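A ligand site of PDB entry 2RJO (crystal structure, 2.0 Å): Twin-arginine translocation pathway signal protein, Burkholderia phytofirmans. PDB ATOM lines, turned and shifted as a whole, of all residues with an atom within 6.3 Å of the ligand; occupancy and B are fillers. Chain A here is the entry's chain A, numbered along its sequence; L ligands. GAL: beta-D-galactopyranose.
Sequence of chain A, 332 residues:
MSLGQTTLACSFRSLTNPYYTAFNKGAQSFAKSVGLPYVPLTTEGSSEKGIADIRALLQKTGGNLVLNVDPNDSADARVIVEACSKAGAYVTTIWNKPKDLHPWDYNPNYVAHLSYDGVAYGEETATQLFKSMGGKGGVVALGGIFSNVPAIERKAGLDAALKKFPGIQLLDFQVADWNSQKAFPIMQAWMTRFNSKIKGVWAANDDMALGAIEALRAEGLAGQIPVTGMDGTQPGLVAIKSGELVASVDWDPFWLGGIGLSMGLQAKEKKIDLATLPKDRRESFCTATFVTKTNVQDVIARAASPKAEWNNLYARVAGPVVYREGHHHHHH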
ATOM      1  N   ARG A  13     -22.761  -6.338 -21.495  1.00  0.00           N
ATOM      2  CA  ARG A  13     -23.309  -7.356 -22.371  1.00  0.00           C
ATOM      3  C   ARG A  13     -23.884  -8.625 -21.730  1.00  0.00           C
ATOM      4  O   ARG A  13     -25.068  -8.910 -21.915  1.00  0.00           O
ATOM      5  CB  ARG A  13     -22.274  -7.730 -23.442  1.00  0.00           C
ATOM      6  CG  ARG A  13     -22.893  -8.123 -24.776  1.00  0.00           C
ATOM      7  CD  ARG A  13     -21.864  -8.260 -25.879  1.00  0.00           C
ATOM      8  NE  ARG A  13     -21.249  -6.997 -26.279  1.00  0.00           N
ATOM      9  CZ  ARG A  13     -20.073  -6.561 -25.835  1.00  0.00           C
ATOM     10  NH1 ARG A  13     -19.377  -7.289 -24.962  1.00  0.00           N
ATOM     11  NH2 ARG A  13     -19.576  -5.416 -26.282  1.00  0.00           N
ATOM     12  N   ASN A  17     -20.041 -14.359 -19.347  1.00  0.00           N
ATOM     13  CA  ASN A  17     -18.597 -14.155 -19.505  1.00  0.00           C
ATOM     14  C   ASN A  17     -18.040 -13.771 -18.141  1.00  0.00           C
ATOM     15  O   ASN A  17     -18.412 -12.733 -17.599  1.00  0.00           O
ATOM     16  CB  ASN A  17     -18.346 -12.997 -20.492  1.00  0.00           C
ATOM     17  CG  ASN A  17     -16.850 -12.731 -20.731  1.00  0.00           C
ATOM     18  OD1 ASN A  17     -16.016 -13.020 -19.878  1.00  0.00           O
ATOM     19  ND2 ASN A  17     -16.535 -12.147 -21.878  1.00  0.00           N
ATOM     20  N   TYR A  19     -15.627 -12.290 -17.288  1.00  0.00           N
ATOM     21  CA  TYR A  19     -15.102 -10.939 -17.295  1.00  0.00           C
ATOM     22  C   TYR A  19     -16.147 -10.005 -16.666  1.00  0.00           C
ATOM     23  O   TYR A  19     -15.839  -9.222 -15.779  1.00  0.00           O
ATOM     24  CB  TYR A  19     -14.810 -10.478 -18.733  1.00  0.00           C
ATOM     25  CG  TYR A  19     -14.542  -8.992 -18.831  1.00  0.00           C
ATOM     26  CD1 TYR A  19     -13.277  -8.469 -18.548  1.00  0.00           C
ATOM     27  CD2 TYR A  19     -15.569  -8.115 -19.144  1.00  0.00           C
ATOM     28  CE1 TYR A  19     -13.050  -7.093 -18.581  1.00  0.00           C
ATOM     29  CE2 TYR A  19     -15.355  -6.732 -19.178  1.00  0.00           C
ATOM     30  CZ  TYR A  19     -14.098  -6.225 -18.891  1.00  0.00           C
ATOM     31  OH  TYR A  19     -13.906  -4.859 -18.930  1.00  0.00           O
ATOM     32  N   TYR A  20     -17.385 -10.118 -17.137  1.00  0.00           N
ATOM     33  CA  TYR A  20     -18.485  -9.308 -16.657  1.00  0.00           C
ATOM     34  C   TYR A  20     -19.010  -9.732 -15.293  1.00  0.00           C
ATOM     35  O   TYR A  20     -19.641  -8.935 -14.596  1.00  0.00           O
ATOM     36  CB  TYR A  20     -19.630  -9.319 -17.685  1.00  0.00           C
ATOM     37  CG  TYR A  20     -19.324  -8.480 -18.910  1.00  0.00           C
ATOM     38  CD1 TYR A  20     -19.375  -9.033 -20.189  1.00  0.00           C
ATOM     39  CD2 TYR A  20     -18.979  -7.130 -18.781  1.00  0.00           C
ATOM     40  CE1 TYR A  20     -19.092  -8.254 -21.317  1.00  0.00           C
ATOM     41  CE2 TYR A  20     -18.683  -6.357 -19.908  1.00  0.00           C
ATOM     42  CZ  TYR A  20     -18.748  -6.920 -21.172  1.00  0.00           C
ATOM     43  OH  TYR A  20     -18.461  -6.163 -22.278  1.00  0.00           O
ATOM     44  N   ASP A  70     -20.401  -0.294 -20.386  1.00  0.00           N
ATOM     45  CA  ASP A  70     -19.516  -0.898 -21.378  1.00  0.00           C
ATOM     46  C   ASP A  70     -20.462  -1.030 -22.586  1.00  0.00           C
ATOM     47  O   ASP A  70     -21.185  -2.018 -22.688  1.00  0.00           O
ATOM     48  CB  ASP A  70     -19.063  -2.280 -20.901  1.00  0.00           C
ATOM     49  CG  ASP A  70     -18.132  -3.001 -21.880  1.00  0.00           C
ATOM     50  OD1 ASP A  70     -18.208  -2.748 -23.100  1.00  0.00           O
ATOM     51  OD2 ASP A  70     -17.320  -3.835 -21.421  1.00  0.00           O
ATOM     52  N   PRO A  71     -20.494  -0.032 -23.491  1.00  0.00           N
ATOM     53  CA  PRO A  71     -21.360  -0.065 -24.665  1.00  0.00           C
ATOM     54  C   PRO A  71     -21.226  -1.329 -25.511  1.00  0.00           C
ATOM     55  O   PRO A  71     -20.117  -1.726 -25.869  1.00  0.00           O
ATOM     56  CB  PRO A  71     -20.949   1.188 -25.438  1.00  0.00           C
ATOM     57  CG  PRO A  71     -20.586   2.126 -24.346  1.00  0.00           C
ATOM     58  CD  PRO A  71     -19.751   1.247 -23.441  1.00  0.00           C
ATOM     59  N   ASN A  72     -22.370  -1.950 -25.808  1.00  0.00           N
ATOM     60  CA  ASN A  72     -22.430  -3.167 -26.621  1.00  0.00           C
ATOM     61  C   ASN A  72     -21.669  -2.948 -27.932  1.00  0.00           C
ATOM     62  O   ASN A  72     -20.931  -3.829 -28.392  1.00  0.00           O
ATOM     63  CB  ASN A  72     -23.890  -3.519 -26.907  1.00  0.00           C
ATOM     64  CG  ASN A  72     -24.046  -4.775 -27.720  1.00  0.00           C
ATOM     65  OD1 ASN A  72     -23.537  -5.836 -27.352  1.00  0.00           O
ATOM     66  ND2 ASN A  72     -24.780  -4.676 -28.839  1.00  0.00           N
ATOM     67  N   ILE A  94     -16.735   2.536 -20.895  1.00  0.00           N
ATOM     68  CA  ILE A  94     -15.660   1.562 -20.836  1.00  0.00           C
ATOM     69  C   ILE A  94     -15.498   0.860 -22.183  1.00  0.00           C
ATOM     70  O   ILE A  94     -16.476   0.353 -22.726  1.00  0.00           O
ATOM     71  CB  ILE A  94     -15.935   0.454 -19.789  1.00  0.00           C
ATOM     72  CG1 ILE A  94     -16.360   1.071 -18.455  1.00  0.00           C
ATOM     73  CG2 ILE A  94     -14.685  -0.389 -19.586  1.00  0.00           C
ATOM     74  CD1 ILE A  94     -15.254   1.830 -17.758  1.00  0.00           C
ATOM     75  N   TRP A  95     -14.283   0.844 -22.713  1.00  0.00           N
ATOM     76  CA  TRP A  95     -14.002   0.149 -23.977  1.00  0.00           C
ATOM     77  C   TRP A  95     -14.522   0.708 -25.296  1.00  0.00           C
ATOM     78  O   TRP A  95     -13.733   1.139 -26.144  1.00  0.00           O
ATOM     79  CB  TRP A  95     -14.459  -1.308 -23.887  1.00  0.00           C
ATOM     80  CG  TRP A  95     -13.665  -2.221 -22.963  1.00  0.00           C
ATOM     81  CD1 TRP A  95     -14.154  -3.001 -21.954  1.00  0.00           C
ATOM     82  CD2 TRP A  95     -12.239  -2.430 -22.962  1.00  0.00           C
ATOM     83  NE1 TRP A  95     -13.136  -3.681 -21.326  1.00  0.00           N
ATOM     84  CE2 TRP A  95     -11.952  -3.352 -21.929  1.00  0.00           C
ATOM     85  CE3 TRP A  95     -11.187  -1.933 -23.734  1.00  0.00           C
ATOM     86  CZ2 TRP A  95     -10.649  -3.781 -21.650  1.00  0.00           C
ATOM     87  CZ3 TRP A  95      -9.883  -2.362 -23.456  1.00  0.00           C
ATOM     88  CH2 TRP A  95      -9.635  -3.266 -22.427  1.00  0.00           C
ATOM     89  N   ASN A  96     -15.840   0.694 -25.488  1.00  0.00           N
ATOM     90  CA  ASN A  96     -16.430   1.107 -26.767  1.00  0.00           C
ATOM     91  C   ASN A  96     -17.036   2.517 -26.884  1.00  0.00           C
ATOM     92  O   ASN A  96     -17.849   2.927 -26.057  1.00  0.00           O
ATOM     93  CB  ASN A  96     -17.494   0.091 -27.206  1.00  0.00           C
ATOM     94  CG  ASN A  96     -16.979  -1.333 -27.233  1.00  0.00           C
ATOM     95  OD1 ASN A  96     -16.027  -1.649 -27.954  1.00  0.00           O
ATOM     96  ND2 ASN A  96     -17.609  -2.210 -26.472  1.00  0.00           N
ATOM     97  N   ASN A 148     -16.232  -3.361 -32.231  1.00  0.00           N
ATOM     98  CA  ASN A 148     -15.732  -2.990 -30.894  1.00  0.00           C
ATOM     99  C   ASN A 148     -14.307  -2.453 -30.942  1.00  0.00           C
ATOM    100  O   ASN A 148     -13.434  -3.019 -31.605  1.00  0.00           O
ATOM    101  CB  ASN A 148     -15.783  -4.200 -29.951  1.00  0.00           C
ATOM    102  CG  ASN A 148     -17.163  -4.429 -29.351  1.00  0.00           C
ATOM    103  OD1 ASN A 148     -18.178  -4.038 -29.923  1.00  0.00           O
ATOM    104  ND2 ASN A 148     -17.195  -5.075 -28.195  1.00  0.00           N
ATOM    105  N   PRO A 150     -11.892  -2.512 -28.658  1.00  0.00           N
ATOM    106  CA  PRO A 150     -10.820  -3.415 -28.218  1.00  0.00           C
ATOM    107  C   PRO A 150     -10.576  -4.555 -29.212  1.00  0.00           C
ATOM    108  O   PRO A 150      -9.455  -5.030 -29.364  1.00  0.00           O
ATOM    109  CB  PRO A 150     -11.293  -3.892 -26.833  1.00  0.00           C
ATOM    110  CG  PRO A 150     -12.782  -3.811 -26.932  1.00  0.00           C
ATOM    111  CD  PRO A 150     -12.999  -2.510 -27.685  1.00  0.00           C
ATOM    112  N   ALA A 151     -11.626  -4.980 -29.899  1.00  0.00           N
ATOM    113  CA  ALA A 151     -11.501  -6.056 -30.887  1.00  0.00           C
ATOM    114  C   ALA A 151     -10.608  -5.591 -32.039  1.00  0.00           C
ATOM    115  O   ALA A 151      -9.770  -6.344 -32.530  1.00  0.00           O
ATOM    116  CB  ALA A 151     -12.880  -6.430 -31.427  1.00  0.00           C
ATOM    117  N   ARG A 154      -6.806  -4.947 -30.468  1.00  0.00           N
ATOM    118  CA  ARG A 154      -6.096  -6.202 -30.163  1.00  0.00           C
ATOM    119  C   ARG A 154      -5.712  -6.934 -31.455  1.00  0.00           C
ATOM    120  O   ARG A 154      -4.612  -7.484 -31.583  1.00  0.00           O
ATOM    121  CB  ARG A 154      -6.969  -7.087 -29.281  1.00  0.00           C
ATOM    122  CG  ARG A 154      -7.308  -6.433 -27.942  1.00  0.00           C
ATOM    123  CD  ARG A 154      -8.358  -7.190 -27.129  1.00  0.00           C
ATOM    124  NE  ARG A 154      -8.800  -6.398 -25.981  1.00  0.00           N
ATOM    125  CZ  ARG A 154      -9.712  -6.781 -25.095  1.00  0.00           C
ATOM    126  NH1 ARG A 154     -10.313  -7.962 -25.189  1.00  0.00           N
ATOM    127  NH2 ARG A 154     -10.026  -5.963 -24.089  1.00  0.00           N
ATOM    128  N   ASP A 177     -17.284 -13.149 -31.569  1.00  0.00           N
ATOM    129  CA  ASP A 177     -18.026 -12.217 -30.736  1.00  0.00           C
ATOM    130  C   ASP A 177     -17.833 -12.343 -29.216  1.00  0.00           C
ATOM    131  O   ASP A 177     -18.825 -12.283 -28.472  1.00  0.00           O
ATOM    132  CB  ASP A 177     -19.537 -12.338 -31.032  1.00  0.00           C
ATOM    133  CG  ASP A 177     -19.904 -11.953 -32.461  1.00  0.00           C
ATOM    134  OD1 ASP A 177     -19.260 -11.052 -33.048  1.00  0.00           O
ATOM    135  OD2 ASP A 177     -20.860 -12.549 -33.009  1.00  0.00           O
ATOM    136  N   TRP A 178     -16.603 -12.530 -28.763  1.00  0.00           N
ATOM    137  CA  TRP A 178     -16.284 -12.657 -27.329  1.00  0.00           C
ATOM    138  C   TRP A 178     -16.931 -13.861 -26.612  1.00  0.00           C
ATOM    139  O   TRP A 178     -16.789 -14.005 -25.407  1.00  0.00           O
ATOM    140  CB  TRP A 178     -16.739 -11.402 -26.569  1.00  0.00           C
ATOM    141  CG  TRP A 178     -16.353 -10.078 -27.186  1.00  0.00           C
ATOM    142  CD1 TRP A 178     -17.203  -9.083 -27.560  1.00  0.00           C
ATOM    143  CD2 TRP A 178     -15.017  -9.575 -27.404  1.00  0.00           C
ATOM    144  NE1 TRP A 178     -16.491  -7.993 -27.996  1.00  0.00           N
ATOM    145  CE2 TRP A 178     -15.150  -8.267 -27.915  1.00  0.00           C
ATOM    146  CE3 TRP A 178     -13.738 -10.099 -27.225  1.00  0.00           C
ATOM    147  CZ2 TRP A 178     -14.037  -7.474 -28.246  1.00  0.00           C
ATOM    148  CZ3 TRP A 178     -12.633  -9.321 -27.553  1.00  0.00           C
ATOM    149  CH2 TRP A 178     -12.796  -8.011 -28.057  1.00  0.00           C
ATOM    150  N   ALA A 204      -8.839 -13.076 -28.850  1.00  0.00           N
ATOM    151  CA  ALA A 204      -8.991 -11.674 -28.458  1.00  0.00           C
ATOM    152  C   ALA A 204      -9.427 -11.460 -26.992  1.00  0.00           C
ATOM    153  O   ALA A 204      -9.362 -10.348 -26.499  1.00  0.00           O
ATOM    154  CB  ALA A 204      -9.960 -10.964 -29.410  1.00  0.00           C
ATOM    155  N   ASN A 205      -9.885 -12.518 -26.326  1.00  0.00           N
ATOM    156  CA  ASN A 205     -10.262 -12.445 -24.900  1.00  0.00           C
ATOM    157  C   ASN A 205     -10.236 -13.843 -24.290  1.00  0.00           C
ATOM    158  O   ASN A 205     -10.100 -14.830 -25.022  1.00  0.00           O
ATOM    159  CB  ASN A 205     -11.643 -11.765 -24.733  1.00  0.00           C
ATOM    160  CG  ASN A 205     -12.810 -12.710 -24.946  1.00  0.00           C
ATOM    161  OD1 ASN A 205     -12.768 -13.576 -25.811  1.00  0.00           O
ATOM    162  ND2 ASN A 205     -13.872 -12.508 -24.188  1.00  0.00           N
ATOM    163  N   ASP A 206     -10.322 -13.944 -22.964  1.00  0.00           N
ATOM    164  CA  ASP A 206     -10.276 -15.250 -22.308  1.00  0.00           C
ATOM    165  C   ASP A 206     -11.412 -16.210 -22.646  1.00  0.00           C
ATOM    166  O   ASP A 206     -11.187 -17.399 -22.826  1.00  0.00           O
ATOM    167  CB  ASP A 206     -10.211 -15.106 -20.783  1.00  0.00           C
ATOM    168  CG  ASP A 206      -8.870 -14.590 -20.301  1.00  0.00           C
ATOM    169  OD1 ASP A 206      -7.945 -14.473 -21.127  1.00  0.00           O
ATOM    170  OD2 ASP A 206      -8.746 -14.308 -19.095  1.00  0.00           O
ATOM    171  N   ASP A 207     -12.640 -15.696 -22.700  1.00  0.00           N
ATOM    172  CA  ASP A 207     -13.780 -16.533 -22.987  1.00  0.00           C
ATOM    173  C   ASP A 207     -13.592 -17.321 -24.286  1.00  0.00           C
ATOM    174  O   ASP A 207     -13.828 -18.524 -24.309  1.00  0.00           O
ATOM    175  CB  ASP A 207     -15.062 -15.710 -23.057  1.00  0.00           C
ATOM    176  CG  ASP A 207     -16.290 -16.489 -22.613  1.00  0.00           C
ATOM    177  OD1 ASP A 207     -16.275 -17.041 -21.494  1.00  0.00           O
ATOM    178  OD2 ASP A 207     -17.286 -16.552 -23.376  1.00  0.00           O
ATOM    179  N   MET A 230      -7.155 -12.758 -23.136  1.00  0.00           N
ATOM    180  CA  MET A 230      -7.057 -11.427 -22.554  1.00  0.00           C
ATOM    181  C   MET A 230      -8.263 -11.180 -21.661  1.00  0.00           C
ATOM    182  O   MET A 230      -9.379 -11.471 -22.053  1.00  0.00           O
ATOM    183  CB  MET A 230      -6.987 -10.338 -23.658  1.00  0.00           C
ATOM    184  CG  MET A 230      -5.565  -9.983 -24.063  1.00  0.00           C
ATOM    185  SD  MET A 230      -5.394  -8.625 -25.268  1.00  0.00           S
ATOM    186  CE  MET A 230      -5.279  -9.543 -26.777  1.00  0.00           C
ATOM    187  N   ASP A 231      -7.994 -10.653 -20.475  1.00  0.00           N
ATOM    188  CA  ASP A 231      -9.020 -10.344 -19.472  1.00  0.00           C
ATOM    189  C   ASP A 231      -8.489 -10.686 -18.084  1.00  0.00           C
ATOM    190  O   ASP A 231      -8.706  -9.946 -17.135  1.00  0.00           O
ATOM    191  CB  ASP A 231     -10.319 -11.122 -19.720  1.00  0.00           C
ATOM    192  CG  ASP A 231     -11.230 -10.443 -20.748  1.00  0.00           C
ATOM    193  OD1 ASP A 231     -10.944  -9.278 -21.113  1.00  0.00           O
ATOM    194  OD2 ASP A 231     -12.222 -11.058 -21.191  1.00  0.00           O
ATOM    195  N   TRP A 251      -7.242  -6.835 -16.913  1.00  0.00           N
ATOM    196  CA  TRP A 251      -7.783  -5.478 -16.984  1.00  0.00           C
ATOM    197  C   TRP A 251      -8.379  -5.147 -15.626  1.00  0.00           C
ATOM    198  O   TRP A 251      -8.680  -3.996 -15.338  1.00  0.00           O
ATOM    199  CB  TRP A 251      -8.922  -5.388 -18.013  1.00  0.00           C
ATOM    200  CG  TRP A 251      -8.671  -6.016 -19.363  1.00  0.00           C
ATOM    201  CD1 TRP A 251      -9.504  -6.899 -20.000  1.00  0.00           C
ATOM    202  CD2 TRP A 251      -7.622  -5.721 -20.295  1.00  0.00           C
ATOM    203  NE1 TRP A 251      -9.034  -7.158 -21.271  1.00  0.00           N
ATOM    204  CE2 TRP A 251      -7.880  -6.448 -21.474  1.00  0.00           C
ATOM    205  CE3 TRP A 251      -6.486  -4.903 -20.250  1.00  0.00           C
ATOM    206  CZ2 TRP A 251      -7.049  -6.392 -22.602  1.00  0.00           C
ATOM    207  CZ3 TRP A 251      -5.652  -4.840 -21.372  1.00  0.00           C
ATOM    208  CH2 TRP A 251      -5.942  -5.579 -22.528  1.00  0.00           C
HETATM  209  C1  GAL L   1     -15.884  -8.397 -23.435  1.00  0.00           C
HETATM  210  C2  GAL L   1     -14.386  -8.761 -23.449  1.00  0.00           C
HETATM  211  C3  GAL L   1     -13.577  -7.526 -22.983  1.00  0.00           C
HETATM  212  C4  GAL L   1     -13.861  -6.353 -23.934  1.00  0.00           C
HETATM  213  C5  GAL L   1     -15.393  -6.089 -23.882  1.00  0.00           C
HETATM  214  C6  GAL L   1     -15.718  -4.951 -24.813  1.00  0.00           C
HETATM  215  O1  GAL L   1     -16.643  -9.534 -23.885  1.00  0.00           O
HETATM  216  O2  GAL L   1     -14.143  -9.848 -22.555  1.00  0.00           O
HETATM  217  O3  GAL L   1     -12.178  -7.821 -23.018  1.00  0.00           O
HETATM  218  O4  GAL L   1     -13.489  -6.741 -25.261  1.00  0.00           O
HETATM  219  O5  GAL L   1     -16.141  -7.268 -24.322  1.00  0.00           O
HETATM  220  O6  GAL L   1     -17.110  -4.715 -24.736  1.00  0.00           O
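Tyr 19 touches the ligand.
CD1 of Trp 95 touches C6 of the ligand (3.8 Å).
Pro 150 touches the ligand.
Trp 178 touches the ligand (CZ2 to O4, 3.1 Å).
NE1 of Trp 251 touches O3 of the ligand, at 3.7 Å.
Hydrophobic or aromatic side chains that line the ligand: Tyr 19, Tyr 20, Trp 95, Pro 150 and Trp 178.
Along chain A the residues within 4 Å of the ligand span positions 13 to 251.
An oxygen (O2) of the ligand is in hydrogen-bond range of the side-chain carboxylate of Asp 231, 2.6 Å away.
OD1 of Asp 70 sits at hydrogen-bond distance from O6 of the ligand.
The guanidinium group (NH1) of Arg 154 sits at hydrogen-bond distance from an oxygen (O3) of the ligand (2.9 Å).
O6 of the ligand lies within hydrogen-bond range of NH2 of Arg 13, 3.0 Å away.
The side-chain amide nitrogen of Asn 96 is in hydrogen-bond range of an oxygen (O6) of the ligand (3.1 Å).
An oxygen (O2) of the ligand lies within hydrogen-bond range of the side-chain amide nitrogen (ND2) of Asn 205 (3.1 Å).
The side-chain hydroxyl of Tyr 20 lies within hydrogen-bond range of an oxygen (O6) of the ligand (3.2 Å).
ND2 of Asn 17 lies within hydrogen-bond range of O1 of the ligand (3.3 Å).
The side-chain amide nitrogen (ND2) of Asn 148 sits at hydrogen-bond distance from an oxygen (O6) of the ligand.
The side-chain carboxylate (OD1) of Asp 231 lies within hydrogen-bond range of the indole nitrogen (NE1) of Trp 251 (2.9 Å).
The side-chain hydroxyl (OH) of Tyr 20 lies within hydrogen-bond range of the side-chain carboxylate (OD2) of Asp 70, at 2.7 Å.
NH1 of Arg 154 lies within hydrogen-bond range of O of Ala 204 (2.9 Å).
The guanidinium group of Arg 13 sits at hydrogen-bond distance from the side-chain amide oxygen of Asn 72 (2.8 Å).
The backbone carbonyl oxygen of Trp 178 is in hydrogen-bond range of the side-chain amide nitrogen of Asn 205.
The side-chain amide nitrogen (ND2) of Asn 148 lies close to the indole nitrogen (NE1) of Trp 178, at 3.0 Å.
The backbone NH (N) of Tyr 19 is in hydrogen-bond range of the side-chain amide oxygen (OD1) of Asn 17 (2.7 Å).
The side-chain amide oxygen (OD1) of Asn 148 lies close to the backbone carbonyl oxygen (O) of Asn 72, at 3.2 Å.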
